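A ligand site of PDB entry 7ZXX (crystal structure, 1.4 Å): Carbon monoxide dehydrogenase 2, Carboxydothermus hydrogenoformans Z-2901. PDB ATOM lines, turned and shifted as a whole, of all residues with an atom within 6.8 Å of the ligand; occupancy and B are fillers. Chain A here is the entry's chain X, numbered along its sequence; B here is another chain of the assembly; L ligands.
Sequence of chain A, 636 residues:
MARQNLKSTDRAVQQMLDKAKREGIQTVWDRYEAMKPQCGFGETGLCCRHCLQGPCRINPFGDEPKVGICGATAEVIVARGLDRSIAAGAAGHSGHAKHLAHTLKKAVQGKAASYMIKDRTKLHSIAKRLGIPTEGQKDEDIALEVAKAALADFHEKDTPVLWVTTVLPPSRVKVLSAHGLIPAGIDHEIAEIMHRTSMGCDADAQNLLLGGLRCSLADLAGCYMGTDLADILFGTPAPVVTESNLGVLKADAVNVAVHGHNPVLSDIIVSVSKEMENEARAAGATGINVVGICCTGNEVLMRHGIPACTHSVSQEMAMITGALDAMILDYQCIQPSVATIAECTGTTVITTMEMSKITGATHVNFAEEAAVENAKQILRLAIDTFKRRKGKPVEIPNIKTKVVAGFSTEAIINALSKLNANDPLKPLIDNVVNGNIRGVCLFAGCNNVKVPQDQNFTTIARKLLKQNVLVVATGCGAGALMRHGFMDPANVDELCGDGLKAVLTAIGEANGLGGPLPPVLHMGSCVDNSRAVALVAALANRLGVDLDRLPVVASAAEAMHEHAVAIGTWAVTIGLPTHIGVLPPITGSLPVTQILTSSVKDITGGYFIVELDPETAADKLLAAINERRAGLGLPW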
ATOM      1  N   CYS A  47      30.507   4.029   8.902  1.00  0.00           N
ATOM      2  CA  CYS A  47      29.644   5.191   8.822  1.00  0.00           C
ATOM      3  C   CYS A  47      28.673   4.938   7.674  1.00  0.00           C
ATOM      4  O   CYS A  47      29.064   4.428   6.616  1.00  0.00           O
ATOM      5  CB  CYS A  47      30.412   6.480   8.562  1.00  0.00           C
ATOM      6  SG  CYS A  47      29.324   7.911   8.428  1.00  0.00           S
ATOM      7  N   CYS A  48      27.399   5.316   7.904  1.00  0.00           N
ATOM      8  CA  CYS A  48      26.352   5.196   6.885  1.00  0.00           C
ATOM      9  C   CYS A  48      25.535   6.482   6.855  1.00  0.00           C
ATOM     10  O   CYS A  48      25.094   6.973   7.906  1.00  0.00           O
ATOM     11  CB  CYS A  48      25.438   4.030   7.225  1.00  0.00           C
ATOM     12  SG  CYS A  48      24.148   3.769   5.991  1.00  0.00           S
ATOM     13  N   ARG A  49      25.319   7.017   5.646  1.00  0.00           N
ATOM     14  CA  ARG A  49      24.429   8.141   5.397  1.00  0.00           C
ATOM     15  C   ARG A  49      23.385   7.780   4.351  1.00  0.00           C
ATOM     16  O   ARG A  49      22.929   8.637   3.597  1.00  0.00           O
ATOM     17  CB  ARG A  49      25.238   9.359   4.955  1.00  0.00           C
ATOM     18  CG  ARG A  49      26.142   9.849   6.054  1.00  0.00           C
ATOM     19  CD  ARG A  49      27.134  10.843   5.518  1.00  0.00           C
ATOM     20  NE  ARG A  49      26.444  11.974   4.939  1.00  0.00           N
ATOM     21  CZ  ARG A  49      26.969  12.809   4.066  1.00  0.00           C
ATOM     22  NH1 ARG A  49      28.232  12.679   3.649  1.00  0.00           N
ATOM     23  NH2 ARG A  49      26.213  13.798   3.598  1.00  0.00           N
ATOM     24  N   HIS A  50      22.971   6.517   4.303  1.00  0.00           N
ATOM     25  CA  HIS A  50      22.034   6.091   3.261  1.00  0.00           C
ATOM     26  C   HIS A  50      20.575   6.435   3.553  1.00  0.00           C
ATOM     27  O   HIS A  50      19.725   6.142   2.713  1.00  0.00           O
ATOM     28  CB  HIS A  50      22.161   4.592   2.960  1.00  0.00           C
ATOM     29  CG  HIS A  50      23.473   4.222   2.350  1.00  0.00           C
ATOM     30  ND1 HIS A  50      23.700   2.991   1.764  1.00  0.00           N
ATOM     31  CD2 HIS A  50      24.633   4.893   2.273  1.00  0.00           C
ATOM     32  CE1 HIS A  50      24.952   2.946   1.332  1.00  0.00           C
ATOM     33  NE2 HIS A  50      25.544   4.087   1.639  1.00  0.00           N
ATOM     34  N   CYS A  51      20.263   7.098   4.661  1.00  0.00           N
ATOM     35  CA  CYS A  51      18.932   7.668   4.821  1.00  0.00           C
ATOM     36  C   CYS A  51      19.012   8.869   5.749  1.00  0.00           C
ATOM     37  O   CYS A  51      20.058   9.124   6.345  1.00  0.00           O
ATOM     38  CB  CYS A  51      17.902   6.641   5.304  1.00  0.00           C
ATOM     39  SG  CYS A  51      17.917   6.315   7.118  1.00  0.00           S
ATOM     40  N   LEU A  52      17.889   9.588   5.875  1.00  0.00           N
ATOM     41  CA  LEU A  52      17.871  10.849   6.617  1.00  0.00           C
ATOM     42  C   LEU A  52      17.742  10.621   8.100  1.00  0.00           C
ATOM     43  O   LEU A  52      17.644  11.604   8.849  1.00  0.00           O
ATOM     44  CB  LEU A  52      16.765  11.774   6.094  1.00  0.00           C
ATOM     45  CG  LEU A  52      16.899  12.155   4.621  1.00  0.00           C
ATOM     46  CD1 LEU A  52      15.673  12.944   4.184  1.00  0.00           C
ATOM     47  CD2 LEU A  52      18.155  12.942   4.397  1.00  0.00           C
ATOM     48  N   GLN A  53      17.721   9.366   8.563  1.00  0.00           N
ATOM     49  CA  GLN A  53      17.884   9.109   9.987  1.00  0.00           C
ATOM     50  C   GLN A  53      19.328   9.186  10.399  1.00  0.00           C
ATOM     51  O   GLN A  53      19.614   9.368  11.593  1.00  0.00           O
ATOM     52  CB  GLN A  53      17.296   7.768  10.409  1.00  0.00           C
ATOM     53  CG  GLN A  53      15.790   7.729  10.257  1.00  0.00           C
ATOM     54  CD  GLN A  53      15.120   6.421  10.564  1.00  0.00           C
ATOM     55  OE1 GLN A  53      14.017   6.427  11.088  1.00  0.00           O
ATOM     56  NE2 GLN A  53      15.741   5.294  10.228  1.00  0.00           N
ATOM     57  N   GLY A  54      20.247   9.093   9.446  1.00  0.00           N
ATOM     58  CA  GLY A  54      21.645   9.196   9.742  1.00  0.00           C
ATOM     59  C   GLY A  54      22.105  10.623   9.952  1.00  0.00           C
ATOM     60  O   GLY A  54      21.316  11.568   9.955  1.00  0.00           O
ATOM     61  N   PRO A  55      23.422  10.828  10.096  1.00  0.00           N
ATOM     62  CA  PRO A  55      24.479   9.816   9.932  1.00  0.00           C
ATOM     63  C   PRO A  55      24.522   8.824  11.068  1.00  0.00           C
ATOM     64  O   PRO A  55      24.318   9.193  12.229  1.00  0.00           O
ATOM     65  CB  PRO A  55      25.774  10.639   9.894  1.00  0.00           C
ATOM     66  CG  PRO A  55      25.392  11.917  10.580  1.00  0.00           C
ATOM     67  CD  PRO A  55      23.977  12.166  10.368  1.00  0.00           C
ATOM     68  N   CYS A  56      24.788   7.561  10.729  1.00  0.00           N
ATOM     69  CA  CYS A  56      25.035   6.525  11.687  1.00  0.00           C
ATOM     70  C   CYS A  56      26.506   6.152  11.651  1.00  0.00           C
ATOM     71  O   CYS A  56      27.147   6.157  10.591  1.00  0.00           O
ATOM     72  CB  CYS A  56      24.200   5.297  11.361  1.00  0.00           C
ATOM     73  SG  CYS A  56      22.413   5.530  11.675  1.00  0.00           S
ATOM     74  N   ARG A  57      27.041   5.828  12.805  1.00  0.00           N
ATOM     75  CA  ARG A  57      28.413   5.364  12.919  1.00  0.00           C
ATOM     76  C   ARG A  57      28.425   4.222  13.929  1.00  0.00           C
ATOM     77  O   ARG A  57      27.500   4.065  14.725  1.00  0.00           O
ATOM     78  CB  ARG A  57      29.348   6.494  13.367  1.00  0.00           C
ATOM     79  CG  ARG A  57      29.109   6.859  14.792  1.00  0.00           C
ATOM     80  CD  ARG A  57      29.725   8.157  15.202  1.00  0.00           C
ATOM     81  NE  ARG A  57      29.492   8.351  16.630  1.00  0.00           N
ATOM     82  CZ  ARG A  57      28.321   8.729  17.171  1.00  0.00           C
ATOM     83  NH1 ARG A  57      28.271   8.791  18.495  1.00  0.00           N
ATOM     84  NH2 ARG A  57      27.215   9.043  16.449  1.00  0.00           N
ATOM     85  N   VAL A  67      25.465  -0.424  16.382  1.00  0.00           N
ATOM     86  CA  VAL A  67      24.614  -0.839  15.280  1.00  0.00           C
ATOM     87  C   VAL A  67      23.940   0.415  14.729  1.00  0.00           C
ATOM     88  O   VAL A  67      23.703   1.378  15.472  1.00  0.00           O
ATOM     89  CB  VAL A  67      23.602  -1.891  15.799  1.00  0.00           C
ATOM     90  CG1 VAL A  67      22.707  -1.301  16.903  1.00  0.00           C
ATOM     91  CG2 VAL A  67      22.749  -2.443  14.713  1.00  0.00           C
ATOM     92  N   GLY A  68      23.610   0.397  13.447  1.00  0.00           N
ATOM     93  CA  GLY A  68      22.887   1.511  12.864  1.00  0.00           C
ATOM     94  C   GLY A  68      21.479   1.631  13.410  1.00  0.00           C
ATOM     95  O   GLY A  68      20.913   0.690  13.985  1.00  0.00           O
ATOM     96  N   ILE A  69      20.883   2.807  13.185  1.00  0.00           N
ATOM     97  CA  ILE A  69      19.563   3.102  13.734  1.00  0.00           C
ATOM     98  C   ILE A  69      18.515   2.099  13.229  1.00  0.00           C
ATOM     99  O   ILE A  69      17.674   1.625  13.994  1.00  0.00           O
ATOM    100  CB  ILE A  69      19.181   4.571  13.455  1.00  0.00           C
ATOM    101  CG1 ILE A  69      19.976   5.478  14.401  1.00  0.00           C
ATOM    102  CG2 ILE A  69      17.687   4.773  13.688  1.00  0.00           C
ATOM    103  CD1 ILE A  69      19.890   6.946  14.040  1.00  0.00           C
ATOM    104  N   CYS A  70      18.593   1.737  11.946  1.00  0.00           N
ATOM    105  CA  CYS A  70      17.647   0.772  11.375  1.00  0.00           C
ATOM    106  C   CYS A  70      17.959  -0.679  11.709  1.00  0.00           C
ATOM    107  O   CYS A  70      17.176  -1.561  11.317  1.00  0.00           O
ATOM    108  CB  CYS A  70      17.650   0.911   9.860  1.00  0.00           C
ATOM    109  SG  CYS A  70      19.280   0.575   9.135  1.00  0.00           S
ATOM    110  N   GLY A  71      19.058  -0.946  12.417  1.00  0.00           N
ATOM    111  CA  GLY A  71      19.528  -2.280  12.692  1.00  0.00           C
ATOM    112  C   GLY A  71      20.659  -2.747  11.814  1.00  0.00           C
ATOM    113  O   GLY A  71      21.090  -3.886  11.943  1.00  0.00           O
ATOM    114  N   ALA A  72      21.146  -1.907  10.898  1.00  0.00           N
ATOM    115  CA  ALA A  72      22.220  -2.306  10.006  1.00  0.00           C
ATOM    116  C   ALA A  72      23.478  -2.590  10.827  1.00  0.00           C
ATOM    117  O   ALA A  72      23.946  -1.739  11.593  1.00  0.00           O
ATOM    118  CB  ALA A  72      22.481  -1.210   8.973  1.00  0.00           C
ATOM    119  N   ILE A  77      26.839  -2.340   6.825  1.00  0.00           N
ATOM    120  CA  ILE A  77      27.258  -0.978   6.495  1.00  0.00           C
ATOM    121  C   ILE A  77      28.520  -0.986   5.637  1.00  0.00           C
ATOM    122  O   ILE A  77      28.607  -0.296   4.616  1.00  0.00           O
ATOM    123  CB  ILE A  77      27.431  -0.154   7.796  1.00  0.00           C
ATOM    124  CG1 ILE A  77      26.059   0.121   8.396  1.00  0.00           C
ATOM    125  CG2 ILE A  77      28.257   1.120   7.576  1.00  0.00           C
ATOM    126  CD1 ILE A  77      26.113   0.767   9.774  1.00  0.00           C
ATOM    127  N   ARG A  80      27.764  -2.373   2.082  1.00  0.00           N
ATOM    128  CA  ARG A  80      26.988  -1.443   1.257  1.00  0.00           C
ATOM    129  C   ARG A  80      27.850  -0.299   0.753  1.00  0.00           C
ATOM    130  O   ARG A  80      27.731   0.107  -0.402  1.00  0.00           O
ATOM    131  CB  ARG A  80      25.790  -0.900   2.032  1.00  0.00           C
ATOM    132  CG  ARG A  80      24.741  -1.973   2.369  1.00  0.00           C
ATOM    133  CD  ARG A  80      23.443  -1.413   2.860  1.00  0.00           C
ATOM    134  NE  ARG A  80      23.639  -0.527   4.015  1.00  0.00           N
ATOM    135  CZ  ARG A  80      22.651  -0.172   4.821  1.00  0.00           C
ATOM    136  NH1 ARG A  80      21.415  -0.587   4.608  1.00  0.00           N
ATOM    137  NH2 ARG A  80      22.882   0.638   5.843  1.00  0.00           N
ATOM    138  N   THR A 197      21.610  -1.440  -1.943  1.00  0.00           N
ATOM    139  CA  THR A 197      22.332  -0.805  -0.847  1.00  0.00           C
ATOM    140  C   THR A 197      21.553   0.341  -0.195  1.00  0.00           C
ATOM    141  O   THR A 197      22.033   0.904   0.796  1.00  0.00           O
ATOM    142  CB  THR A 197      23.692  -0.288  -1.310  1.00  0.00           C
ATOM    143  OG1 THR A 197      23.505   0.653  -2.370  1.00  0.00           O
ATOM    144  CG2 THR A 197      24.601  -1.436  -1.763  1.00  0.00           C
ATOM    145  N   SER A 198      20.381   0.690  -0.710  1.00  0.00           N
ATOM    146  CA  SER A 198      19.584   1.709  -0.073  1.00  0.00           C
ATOM    147  C   SER A 198      18.961   1.151   1.203  1.00  0.00           C
ATOM    148  O   SER A 198      19.006  -0.044   1.493  1.00  0.00           O
ATOM    149  CB  SER A 198      18.562   2.305  -1.065  1.00  0.00           C
ATOM    150  OG  SER A 198      17.488   1.427  -1.322  1.00  0.00           O
ATOM    151  N   MET A 199      18.379   2.055   1.990  1.00  0.00           N
ATOM    152  CA  MET A 199      17.908   1.677   3.322  1.00  0.00           C
ATOM    153  C   MET A 199      16.831   0.593   3.266  1.00  0.00           C
ATOM    154  O   MET A 199      15.903   0.623   2.430  1.00  0.00           O
ATOM    155  CB  MET A 199      17.407   2.928   4.065  1.00  0.00           C
ATOM    156  CG  MET A 199      16.887   2.654   5.481  1.00  0.00           C
ATOM    157  SD  MET A 199      15.194   2.049   5.482  1.00  0.00           S
ATOM    158  CE  MET A 199      14.888   1.918   7.227  1.00  0.00           C
ATOM    159  N   GLY A 200      17.005  -0.401   4.136  1.00  0.00           N
ATOM    160  CA  GLY A 200      15.954  -1.393   4.297  1.00  0.00           C
ATOM    161  C   GLY A 200      15.880  -2.385   3.176  1.00  0.00           C
ATOM    162  O   GLY A 200      14.792  -2.936   2.932  1.00  0.00           O
ATOM    163  N   MET B  35      22.923   6.487  19.328  1.00  0.00           N
ATOM    164  CA  MET B  35      23.670   7.159  18.280  1.00  0.00           C
ATOM    165  C   MET B  35      23.906   8.639  18.569  1.00  0.00           C
ATOM    166  O   MET B  35      24.718   9.275  17.883  1.00  0.00           O
ATOM    167  CB  MET B  35      22.903   7.026  16.952  1.00  0.00           C
ATOM    168  CG  MET B  35      23.731   7.297  15.699  1.00  0.00           C
ATOM    169  SD  MET B  35      25.096   6.147  15.509  1.00  0.00           S
ATOM    170  CE  MET B  35      24.212   4.615  15.176  1.00  0.00           C
ATOM    171  N   GLN B  38      24.624  12.773  16.982  1.00  0.00           N
ATOM    172  CA  GLN B  38      25.008  12.352  15.645  1.00  0.00           C
ATOM    173  C   GLN B  38      26.040  13.314  15.037  1.00  0.00           C
ATOM    174  O   GLN B  38      26.149  14.487  15.420  1.00  0.00           O
ATOM    175  CB  GLN B  38      23.767  12.218  14.742  1.00  0.00           C
ATOM    176  CG  GLN B  38      22.841  11.122  15.198  1.00  0.00           C
ATOM    177  CD  GLN B  38      21.631  10.975  14.322  1.00  0.00           C
ATOM    178  OE1 GLN B  38      20.610  11.613  14.550  1.00  0.00           O
ATOM    179  NE2 GLN B  38      21.735  10.107  13.347  1.00  0.00           N
ATOM    180  N   PRO B 336      16.459  -4.011   9.163  1.00  0.00           N
ATOM    181  CA  PRO B 336      17.026  -5.365   9.271  1.00  0.00           C
ATOM    182  C   PRO B 336      17.015  -5.890  10.691  1.00  0.00           C
ATOM    183  O   PRO B 336      17.209  -7.098  10.893  1.00  0.00           O
ATOM    184  CB  PRO B 336      18.435  -5.224   8.676  1.00  0.00           C
ATOM    185  CG  PRO B 336      18.766  -3.780   8.794  1.00  0.00           C
ATOM    186  CD  PRO B 336      17.460  -3.052   8.637  1.00  0.00           C
ATOM    187  N   MET B 560      12.590  10.031   5.184  1.00  0.00           N
ATOM    188  CA  MET B 560      13.688   9.179   5.638  1.00  0.00           C
ATOM    189  C   MET B 560      14.468   8.579   4.470  1.00  0.00           C
ATOM    190  O   MET B 560      15.670   8.786   4.352  1.00  0.00           O
ATOM    191  CB  MET B 560      13.107   8.089   6.534  1.00  0.00           C
ATOM    192  CG  MET B 560      14.125   7.082   7.065  1.00  0.00           C
ATOM    193  SD  MET B 560      14.406   5.589   6.054  1.00  0.00           S
ATOM    194  CE  MET B 560      12.780   4.856   6.110  1.00  0.00           C
HETATM  195 FE1  LIG L   1      21.475   4.763   9.691  1.00  0.00          FE
HETATM  196 FE2  LIG L   1      19.803   5.101   7.607  1.00  0.00          FE
HETATM  197 FE3  LIG L   1      22.231   3.978   7.261  1.00  0.00          FE
HETATM  198 FE4  LIG L   1      20.300   2.557   8.571  1.00  0.00          FE
HETATM  199  S1  LIG L   1      20.319   3.226   6.370  1.00  0.00           S
HETATM  200  S2  LIG L   1      22.447   2.764   9.181  1.00  0.00           S
HETATM  201  S3  LIG L   1      19.300   4.313   9.690  1.00  0.00           S
HETATM  202  S4  LIG L   1      21.773   6.096   7.866  1.00  0.00           S
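An iron atom (FE3) of the ligand is bound by the side-chain sulfur of Cys 48 (2.3 Å). The side-chain sulfur (SG) of Cys 56 binds an iron atom (FE1) of the ligand (2.3 Å). The guanidinium group (NH2) of Arg 80 sits close to a sulfur (S1) of the ligand (3.7 Å). The side-chain sulfur (SG) of Cys 51 binds an iron atom (FE2) of the ligand, at 2.3 Å. An iron atom (FE4) of the ligand is bound by the side-chain sulfur of Cys 70 (2.3 Å). A sulfur (S4) of the ligand lies close to the backbone NH (N) of Cys 51 (3.7 Å). N of His 50 sits close to S4 of the ligand, at 3.8 Å. N of Gly 54 sits close to S4 of the ligand (3.7 Å). NE2 of Gln 53 sits close to S3 of the ligand, at 3.7 Å. The backbone NH (N) of Cys 70 sits close to a sulfur (S3) of the ligand.
The side-chain sulfur (SG) of Cys 56 lies close to the backbone NH (N) of Ile 69 (3.5 Å). O of Cys 56 lies close to SG of Cys 47 (3.5 Å). A ring nitrogen (ND1) of His 50 lies within hydrogen-bond range of the backbone carbonyl oxygen (O) of Thr 197, 2.8 Å away. NE2 of Gln 38 of chain B lies within hydrogen-bond range of O of Gln 53. The backbone NH of Cys 48 lies within hydrogen-bond range of the backbone carbonyl oxygen of Cys 56 (2.8 Å). The side-chain sulfur (SG) of Cys 48 sits close to the guanidinium group (NH2) of Arg 80 (3.4 Å). The side-chain sulfur (SG) of Cys 70 lies close to the backbone NH (N) of Ala 72, at 3.6 Å. The side-chain sulfur of Cys 48 lies close to the backbone NH of His 50.
Gly 68 touches the ligand (CA to S2, 3.9 Å). Ile 69 touches the ligand (CB to S3, 3.8 Å). CB of Ala 72 touches S2 of the ligand (3.98 Å). Met 199 touches the ligand (CG to S1, 3.6 Å). Hydrophobic or aromatic side chains within 4 Å of the ligand: Ile 69, Ala 72 and Met 199. Within 4 Å of the ligand: Cys 48, His 50, Cys 51, Gln 53, Gly 54, Cys 56, Gly 68, Ile 69, Cys 70, Ala 72, Arg 80 and Met 199.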
